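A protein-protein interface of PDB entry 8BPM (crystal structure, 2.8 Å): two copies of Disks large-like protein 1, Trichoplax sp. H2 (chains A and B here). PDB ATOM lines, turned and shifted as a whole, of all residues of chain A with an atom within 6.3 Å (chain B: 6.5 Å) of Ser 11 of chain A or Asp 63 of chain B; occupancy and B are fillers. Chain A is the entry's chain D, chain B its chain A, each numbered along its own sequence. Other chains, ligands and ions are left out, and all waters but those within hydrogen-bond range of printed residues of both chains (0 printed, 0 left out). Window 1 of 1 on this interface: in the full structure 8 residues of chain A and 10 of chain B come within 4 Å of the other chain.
Among the printed residues, pairs that only touch across the chains: Pro 10 of chain A with Gly 20 of chain B, Ser 11 of chain A with His 62 of chain B and Phe 30 of chain A with Glu 67 of chain B.
No position is printed for both chains. Of the 12 pairs that touch across the chains among the printed residues, none has its exchanged pair printed and touching as well.
Hydrophobic or aromatic side chains of chain B within 4 Å of the printed part of chain A: His 62. Hydrophobic or aromatic side chains of chain A within 4 Å of the printed part of chain B: Phe 30. Among the printed residues, no Asp or Glu carboxylate lies within 4 Å of a Lys or Arg side-chain nitrogen of the other chain.
The backbone carbonyl oxygen (O) of Gly 19 of chain B lies within hydrogen-bond range of the side-chain hydroxyl (OG) of Ser 11 of chain A (3.2 Å). N of Asp 21 of chain B is in hydrogen-bond range of O of Pro 10 of chain A (3.4 Å). The side-chain carboxylate of Asp 63 of chain B is in hydrogen-bond range of the backbone NH of Gly 14 of chain A. The side-chain carboxylate (OD2) of Asp 63 of chain B lies within hydrogen-bond range of the backbone NH (N) of Phe 15 of chain A, at 3.5 Å. The backbone carbonyl oxygen (O) of Asp 63 of chain B is in hydrogen-bond range of the side-chain amide nitrogen (ND2) of Asn 16 of chain A (3.0 Å). The side-chain hydroxyl of Ser 32 of chain A lies within hydrogen-bond range of the side-chain carboxylate of Asp 63 of chain B (2.8 Å). The side-chain amide oxygen (OD1) of Asn 16 of chain A is in hydrogen-bond range of the backbone NH (N) of Glu 64 of chain B. OE1 of Glu 67 of chain B sits at hydrogen-bond distance from ND2 of Asn 16 of chain A, 2.9 Å away. The backbone carbonyl oxygen of Ser 11 of chain A lies close to the side-chain carboxylate of Asp 63 of chain B (3.2 Å).
Of chain B, only Gly 19 (3.2 Å), His 62 (3.6 Å) and Asp 63 (3.2 Å) come within 4 Å of Ser 11 of chain A. Of chain A, only Ser 11 (3.2 Å), Gly 14 (3.1 Å), Phe 15 (3.5 Å), Asn 16 (3.0 Å) and Ser 32 (2.8 Å) come within 4 Å of Asp 63 of chain B. Of the printed residues of chain A, Glu 64 of chain B touches Asn 16 (3.4 Å). Printed residues of chain B within 4 Å of Asn 16 of chain A: Asp 63, Glu 64 and Glu 67. Gln 24 of chain B touches none of the printed residues of chain A. The nearest residue of chain A that does not touch Asp 63 of chain B is Leu 13 of chain A (4.03 Å). The nearest printed residue of chain B that does not touch Phe 30 of chain A is Val 66 of chain B (4.01 Å).
A ring nitrogen (ND1) of His 62 of chain B sits at hydrogen-bond distance from the backbone NH of Gly 19 of chain B (3.0 Å). The backbone NH of His 62 of chain B sits at hydrogen-bond distance from the backbone carbonyl oxygen of Gly 20 of chain B (3.0 Å). The backbone NH (N) of Asp 21 of chain B lies within hydrogen-bond range of the side-chain amide oxygen (OE1) of Gln 24 of chain B (2.6 Å). The side-chain hydroxyl (OG) of Ser 61 of chain B lies close to the backbone NH (N) of Asp 63 of chain B (3.4 Å). The backbone NH of Ser 61 of chain B is in hydrogen-bond range of the side-chain carboxylate of Glu 64 of chain B (2.9 Å). The backbone carbonyl oxygen of Phe 30 of chain A lies within hydrogen-bond range of the backbone NH of Asn 16 of chain A (2.9 Å).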
ATOM      1  N   ARG A   8      -8.050  -6.696  13.003  1.00  0.00           N
ATOM      2  CA  ARG A   8      -6.768  -7.376  12.910  1.00  0.00           C
ATOM      3  C   ARG A   8      -6.902  -8.834  13.327  1.00  0.00           C
ATOM      4  O   ARG A   8      -7.575  -9.159  14.307  1.00  0.00           O
ATOM      5  CB  ARG A   8      -5.732  -6.662  13.778  1.00  0.00           C
ATOM      6  CG  ARG A   8      -4.323  -7.243  13.655  1.00  0.00           C
ATOM      7  CD  ARG A   8      -3.333  -6.504  14.533  1.00  0.00           C
ATOM      8  NE  ARG A   8      -3.285  -5.085  14.208  1.00  0.00           N
ATOM      9  CZ  ARG A   8      -2.393  -4.522  13.402  1.00  0.00           C
ATOM     10  NH1 ARG A   8      -1.427  -5.230  12.829  1.00  0.00           N
ATOM     11  NH2 ARG A   8      -2.468  -3.212  13.170  1.00  0.00           N
ATOM     12  N   ARG A   9      -6.275  -9.714  12.562  1.00  0.00           N
ATOM     13  CA  ARG A   9      -6.100 -11.118  12.900  1.00  0.00           C
ATOM     14  C   ARG A   9      -4.650 -11.409  13.262  1.00  0.00           C
ATOM     15  O   ARG A   9      -3.761 -10.576  13.051  1.00  0.00           O
ATOM     16  CB  ARG A   9      -6.541 -12.022  11.738  1.00  0.00           C
ATOM     17  CG  ARG A   9      -8.049 -12.166  11.608  1.00  0.00           C
ATOM     18  CD  ARG A   9      -8.454 -13.360  10.736  1.00  0.00           C
ATOM     19  NE  ARG A   9      -9.802 -13.213  10.192  1.00  0.00           N
ATOM     20  CZ  ARG A   9     -10.120 -13.057   8.910  1.00  0.00           C
ATOM     21  NH1 ARG A   9      -9.200 -13.043   7.956  1.00  0.00           N
ATOM     22  NH2 ARG A   9     -11.401 -12.912   8.576  1.00  0.00           N
ATOM     23  N   PRO A  10      -4.380 -12.574  13.857  1.00  0.00           N
ATOM     24  CA  PRO A  10      -2.983 -12.928  14.154  1.00  0.00           C
ATOM     25  C   PRO A  10      -2.084 -12.868  12.932  1.00  0.00           C
ATOM     26  O   PRO A  10      -0.879 -12.612  13.067  1.00  0.00           O
ATOM     27  CB  PRO A  10      -3.101 -14.348  14.719  1.00  0.00           C
ATOM     28  CG  PRO A  10      -4.452 -14.400  15.303  1.00  0.00           C
ATOM     29  CD  PRO A  10      -5.324 -13.559  14.412  1.00  0.00           C
ATOM     30  N   SER A  11      -2.640 -13.093  11.738  1.00  0.00           N
ATOM     31  CA  SER A  11      -1.899 -12.980  10.489  1.00  0.00           C
ATOM     32  C   SER A  11      -1.806 -11.545   9.985  1.00  0.00           C
ATOM     33  O   SER A  11      -1.391 -11.333   8.838  1.00  0.00           O
ATOM     34  CB  SER A  11      -2.550 -13.863   9.423  1.00  0.00           C
ATOM     35  OG  SER A  11      -2.525 -15.223   9.821  1.00  0.00           O
ATOM     36  N   GLY A  12      -2.161 -10.566  10.815  1.00  0.00           N
ATOM     37  CA  GLY A  12      -2.125  -9.172  10.413  1.00  0.00           C
ATOM     38  C   GLY A  12      -3.472  -8.688   9.904  1.00  0.00           C
ATOM     39  O   GLY A  12      -4.527  -9.250  10.212  1.00  0.00           O
ATOM     40  N   LEU A  13      -3.426  -7.616   9.106  1.00  0.00           N
ATOM     41  CA  LEU A  13      -4.619  -7.044   8.488  1.00  0.00           C
ATOM     42  C   LEU A  13      -4.896  -7.593   7.092  1.00  0.00           C
ATOM     43  O   LEU A  13      -5.968  -7.318   6.534  1.00  0.00           O
ATOM     44  CB  LEU A  13      -4.495  -5.521   8.408  1.00  0.00           C
ATOM     45  CG  LEU A  13      -4.381  -4.827   9.759  1.00  0.00           C
ATOM     46  CD1 LEU A  13      -3.924  -3.394   9.557  1.00  0.00           C
ATOM     47  CD2 LEU A  13      -5.713  -4.881  10.497  1.00  0.00           C
ATOM     48  N   GLY A  14      -3.961  -8.342   6.513  1.00  0.00           N
ATOM     49  CA  GLY A  14      -4.169  -8.943   5.215  1.00  0.00           C
ATOM     50  C   GLY A  14      -3.720  -8.111   4.037  1.00  0.00           C
ATOM     51  O   GLY A  14      -4.251  -8.284   2.931  1.00  0.00           O
ATOM     52  N   PHE A  15      -2.757  -7.211   4.232  1.00  0.00           N
ATOM     53  CA  PHE A  15      -2.243  -6.428   3.119  1.00  0.00           C
ATOM     54  C   PHE A  15      -0.881  -5.855   3.484  1.00  0.00           C
ATOM     55  O   PHE A  15      -0.538  -5.727   4.661  1.00  0.00           O
ATOM     56  CB  PHE A  15      -3.224  -5.314   2.713  1.00  0.00           C
ATOM     57  CG  PHE A  15      -3.344  -4.191   3.714  1.00  0.00           C
ATOM     58  CD1 PHE A  15      -4.236  -4.273   4.769  1.00  0.00           C
ATOM     59  CD2 PHE A  15      -2.595  -3.038   3.573  1.00  0.00           C
ATOM     60  CE1 PHE A  15      -4.352  -3.244   5.675  1.00  0.00           C
ATOM     61  CE2 PHE A  15      -2.716  -2.007   4.477  1.00  0.00           C
ATOM     62  CZ  PHE A  15      -3.592  -2.113   5.527  1.00  0.00           C
ATOM     63  N   ASN A  16      -0.090  -5.581   2.447  1.00  0.00           N
ATOM     64  CA  ASN A  16       1.193  -4.902   2.549  1.00  0.00           C
ATOM     65  C   ASN A  16       1.098  -3.548   1.858  1.00  0.00           C
ATOM     66  O   ASN A  16       0.307  -3.368   0.926  1.00  0.00           O
ATOM     67  CB  ASN A  16       2.311  -5.722   1.905  1.00  0.00           C
ATOM     68  CG  ASN A  16       2.453  -7.090   2.517  1.00  0.00           C
ATOM     69  OD1 ASN A  16       2.387  -7.250   3.734  1.00  0.00           O
ATOM     70  ND2 ASN A  16       2.645  -8.093   1.673  1.00  0.00           N
ATOM     71  N   PHE A  30      -0.334  -4.854  -1.863  1.00  0.00           N
ATOM     72  CA  PHE A  30      -0.617  -6.273  -2.010  1.00  0.00           C
ATOM     73  C   PHE A  30      -1.686  -6.665  -1.004  1.00  0.00           C
ATOM     74  O   PHE A  30      -1.704  -6.147   0.112  1.00  0.00           O
ATOM     75  CB  PHE A  30       0.648  -7.106  -1.784  1.00  0.00           C
ATOM     76  CG  PHE A  30       0.437  -8.575  -1.936  1.00  0.00           C
ATOM     77  CD1 PHE A  30       0.480  -9.158  -3.182  1.00  0.00           C
ATOM     78  CD2 PHE A  30       0.200  -9.370  -0.836  1.00  0.00           C
ATOM     79  CE1 PHE A  30       0.292 -10.499  -3.330  1.00  0.00           C
ATOM     80  CE2 PHE A  30       0.012 -10.712  -0.979  1.00  0.00           C
ATOM     81  CZ  PHE A  30       0.058 -11.281  -2.228  1.00  0.00           C
ATOM     82  N   SER A  32      -3.237 -10.068   0.664  1.00  0.00           N
ATOM     83  CA  SER A  32      -3.174 -11.507   0.851  1.00  0.00           C
ATOM     84  C   SER A  32      -4.552 -12.131   0.683  1.00  0.00           C
ATOM     85  O   SER A  32      -5.529 -11.665   1.276  1.00  0.00           O
ATOM     86  CB  SER A  32      -2.646 -11.816   2.246  1.00  0.00           C
ATOM     87  OG  SER A  32      -1.334 -11.327   2.419  1.00  0.00           O
ATOM     88  N   GLY A  35      -7.172 -13.052   3.862  1.00  0.00           N
ATOM     89  CA  GLY A  35      -6.960 -12.162   4.976  1.00  0.00           C
ATOM     90  C   GLY A  35      -8.116 -11.207   5.177  1.00  0.00           C
ATOM     91  O   GLY A  35      -9.079 -11.186   4.404  1.00  0.00           O
ATOM     92  N   PRO A  36      -8.050 -10.403   6.242  1.00  0.00           N
ATOM     93  CA  PRO A  36      -9.140  -9.444   6.497  1.00  0.00           C
ATOM     94  C   PRO A  36      -9.387  -8.470   5.353  1.00  0.00           C
ATOM     95  O   PRO A  36     -10.544  -8.135   5.067  1.00  0.00           O
ATOM     96  CB  PRO A  36      -8.676  -8.723   7.774  1.00  0.00           C
ATOM     97  CG  PRO A  36      -7.767  -9.702   8.451  1.00  0.00           C
ATOM     98  CD  PRO A  36      -7.070 -10.447   7.345  1.00  0.00           C
ATOM     99  N   VAL B  18       1.350 -20.276   6.481  1.00  0.00           N
ATOM    100  CA  VAL B  18       0.705 -19.473   7.509  1.00  0.00           C
ATOM    101  C   VAL B  18       1.785 -18.858   8.384  1.00  0.00           C
ATOM    102  O   VAL B  18       2.796 -19.500   8.691  1.00  0.00           O
ATOM    103  CB  VAL B  18      -0.268 -20.312   8.359  1.00  0.00           C
ATOM    104  CG1 VAL B  18      -1.461 -20.744   7.516  1.00  0.00           C
ATOM    105  CG2 VAL B  18       0.467 -21.513   8.967  1.00  0.00           C
ATOM    106  N   GLY B  19       1.556 -17.614   8.797  1.00  0.00           N
ATOM    107  CA  GLY B  19       2.474 -16.902   9.659  1.00  0.00           C
ATOM    108  C   GLY B  19       1.693 -16.032  10.618  1.00  0.00           C
ATOM    109  O   GLY B  19       0.460 -16.036  10.618  1.00  0.00           O
ATOM    110  N   GLY B  20       2.428 -15.284  11.431  1.00  0.00           N
ATOM    111  CA  GLY B  20       1.795 -14.378  12.363  1.00  0.00           C
ATOM    112  C   GLY B  20       2.200 -12.937  12.151  1.00  0.00           C
ATOM    113  O   GLY B  20       2.178 -12.429  11.025  1.00  0.00           O
ATOM    114  N   ASP B  21       2.539 -12.262  13.240  1.00  0.00           N
ATOM    115  CA  ASP B  21       3.142 -10.944  13.155  1.00  0.00           C
ATOM    116  C   ASP B  21       4.627 -11.109  12.841  1.00  0.00           C
ATOM    117  O   ASP B  21       5.132 -12.223  12.654  1.00  0.00           O
ATOM    118  CB  ASP B  21       2.920 -10.181  14.455  1.00  0.00           C
ATOM    119  CG  ASP B  21       2.838  -8.686  14.250  1.00  0.00           C
ATOM    120  OD1 ASP B  21       3.089  -8.205  13.120  1.00  0.00           O
ATOM    121  OD2 ASP B  21       2.514  -7.993  15.235  1.00  0.00           O
ATOM    122  N   GLN B  24       7.261 -14.038  14.103  1.00  0.00           N
ATOM    123  CA  GLN B  24       6.549 -15.197  14.623  1.00  0.00           C
ATOM    124  C   GLN B  24       6.876 -16.470  13.860  1.00  0.00           C
ATOM    125  O   GLN B  24       6.677 -17.563  14.395  1.00  0.00           O
ATOM    126  CB  GLN B  24       5.036 -14.952  14.596  1.00  0.00           C
ATOM    127  CG  GLN B  24       4.562 -13.898  15.612  1.00  0.00           C
ATOM    128  CD  GLN B  24       3.115 -14.106  16.073  1.00  0.00           C
ATOM    129  OE1 GLN B  24       2.183 -13.499  15.536  1.00  0.00           O
ATOM    130  NE2 GLN B  24       2.928 -14.965  17.075  1.00  0.00           N
ATOM    131  N   ILE B  26       7.309 -18.271   9.624  1.00  0.00           N
ATOM    132  CA  ILE B  26       6.527 -18.619   8.444  1.00  0.00           C
ATOM    133  C   ILE B  26       6.589 -20.130   8.286  1.00  0.00           C
ATOM    134  O   ILE B  26       7.675 -20.702   8.132  1.00  0.00           O
ATOM    135  CB  ILE B  26       7.048 -17.910   7.186  1.00  0.00           C
ATOM    136  CG1 ILE B  26       7.120 -16.394   7.394  1.00  0.00           C
ATOM    137  CG2 ILE B  26       6.169 -18.233   5.997  1.00  0.00           C
ATOM    138  CD1 ILE B  26       5.809 -15.746   7.740  1.00  0.00           C
ATOM    139  N   ALA B  60       9.604 -11.685   9.075  1.00  0.00           N
ATOM    140  CA  ALA B  60       8.503 -11.349   8.185  1.00  0.00           C
ATOM    141  C   ALA B  60       7.144 -11.630   8.822  1.00  0.00           C
ATOM    142  O   ALA B  60       6.982 -12.569   9.607  1.00  0.00           O
ATOM    143  CB  ALA B  60       8.613 -12.131   6.874  1.00  0.00           C
ATOM    144  N   SER B  61       6.165 -10.796   8.463  1.00  0.00           N
ATOM    145  CA  SER B  61       4.769 -11.041   8.785  1.00  0.00           C
ATOM    146  C   SER B  61       4.172 -12.030   7.783  1.00  0.00           C
ATOM    147  O   SER B  61       4.750 -12.318   6.732  1.00  0.00           O
ATOM    148  CB  SER B  61       3.974  -9.734   8.763  1.00  0.00           C
ATOM    149  OG  SER B  61       3.467  -9.462   7.467  1.00  0.00           O
ATOM    150  N   HIS B  62       2.981 -12.539   8.102  1.00  0.00           N
ATOM    151  CA  HIS B  62       2.337 -13.490   7.203  1.00  0.00           C
ATOM    152  C   HIS B  62       2.193 -12.902   5.806  1.00  0.00           C
ATOM    153  O   HIS B  62       2.599 -13.515   4.813  1.00  0.00           O
ATOM    154  CB  HIS B  62       0.963 -13.896   7.737  1.00  0.00           C
ATOM    155  CG  HIS B  62       0.146 -14.674   6.751  1.00  0.00           C
ATOM    156  ND1 HIS B  62       0.104 -16.052   6.739  1.00  0.00           N
ATOM    157  CD2 HIS B  62      -0.644 -14.268   5.731  1.00  0.00           C
ATOM    158  CE1 HIS B  62      -0.682 -16.460   5.761  1.00  0.00           C
ATOM    159  NE2 HIS B  62      -1.151 -15.397   5.135  1.00  0.00           N
ATOM    160  N   ASP B  63       1.596 -11.715   5.709  1.00  0.00           N
ATOM    161  CA  ASP B  63       1.289 -11.157   4.397  1.00  0.00           C
ATOM    162  C   ASP B  63       2.563 -10.841   3.627  1.00  0.00           C
ATOM    163  O   ASP B  63       2.618 -11.011   2.401  1.00  0.00           O
ATOM    164  CB  ASP B  63       0.427  -9.911   4.554  1.00  0.00           C
ATOM    165  CG  ASP B  63      -0.775 -10.151   5.447  1.00  0.00           C
ATOM    166  OD1 ASP B  63      -1.469 -11.167   5.239  1.00  0.00           O
ATOM    167  OD2 ASP B  63      -1.021  -9.321   6.353  1.00  0.00           O
ATOM    168  N   GLU B  64       3.585 -10.350   4.324  1.00  0.00           N
ATOM    169  CA  GLU B  64       4.871 -10.101   3.680  1.00  0.00           C
ATOM    170  C   GLU B  64       5.424 -11.381   3.062  1.00  0.00           C
ATOM    171  O   GLU B  64       5.814 -11.401   1.887  1.00  0.00           O
ATOM    172  CB  GLU B  64       5.838  -9.485   4.696  1.00  0.00           C
ATOM    173  CG  GLU B  64       5.448  -8.032   5.074  1.00  0.00           C
ATOM    174  CD  GLU B  64       6.133  -7.482   6.320  1.00  0.00           C
ATOM    175  OE1 GLU B  64       6.597  -8.261   7.177  1.00  0.00           O
ATOM    176  OE2 GLU B  64       6.216  -6.246   6.427  1.00  0.00           O
ATOM    177  N   ALA B  65       5.428 -12.474   3.828  1.00  0.00           N
ATOM    178  CA  ALA B  65       5.987 -13.723   3.322  1.00  0.00           C
ATOM    179  C   ALA B  65       5.186 -14.246   2.137  1.00  0.00           C
ATOM    180  O   ALA B  65       5.758 -14.756   1.168  1.00  0.00           O
ATOM    181  CB  ALA B  65       6.038 -14.762   4.441  1.00  0.00           C
ATOM    182  N   VAL B  66       3.861 -14.136   2.197  1.00  0.00           N
ATOM    183  CA  VAL B  66       3.028 -14.580   1.083  1.00  0.00           C
ATOM    184  C   VAL B  66       3.406 -13.841  -0.195  1.00  0.00           C
ATOM    185  O   VAL B  66       3.543 -14.442  -1.263  1.00  0.00           O
ATOM    186  CB  VAL B  66       1.540 -14.385   1.421  1.00  0.00           C
ATOM    187  CG1 VAL B  66       0.693 -14.496   0.169  1.00  0.00           C
ATOM    188  CG2 VAL B  66       1.114 -15.397   2.459  1.00  0.00           C
ATOM    189  N   GLU B  67       3.566 -12.519  -0.106  1.00  0.00           N
ATOM    190  CA  GLU B  67       3.929 -11.745  -1.288  1.00  0.00           C
ATOM    191  C   GLU B  67       5.313 -12.118  -1.796  1.00  0.00           C
ATOM    192  O   GLU B  67       5.556 -12.130  -3.007  1.00  0.00           O
ATOM    193  CB  GLU B  67       3.893 -10.247  -0.984  1.00  0.00           C
ATOM    194  CG  GLU B  67       4.336  -9.380  -2.169  1.00  0.00           C
ATOM    195  CD  GLU B  67       4.225  -7.904  -1.881  1.00  0.00           C
ATOM    196  OE1 GLU B  67       4.213  -7.530  -0.689  1.00  0.00           O
ATOM    197  OE2 GLU B  67       4.140  -7.121  -2.851  1.00  0.00           O
ATOM    198  N   ILE B  68       6.256 -12.342  -0.884  1.00  0.00           N
ATOM    199  CA  ILE B  68       7.603 -12.717  -1.300  1.00  0.00           C
ATOM    200  C   ILE B  68       7.568 -14.057  -2.021  1.00  0.00           C
ATOM    201  O   ILE B  68       8.068 -14.194  -3.144  1.00  0.00           O
ATOM    202  CB  ILE B  68       8.552 -12.731  -0.086  1.00  0.00           C
ATOM    203  CG1 ILE B  68       8.812 -11.285   0.372  1.00  0.00           C
ATOM    204  CG2 ILE B  68       9.846 -13.456  -0.423  1.00  0.00           C
ATOM    205  CD1 ILE B  68       9.699 -11.159   1.596  1.00  0.00           C
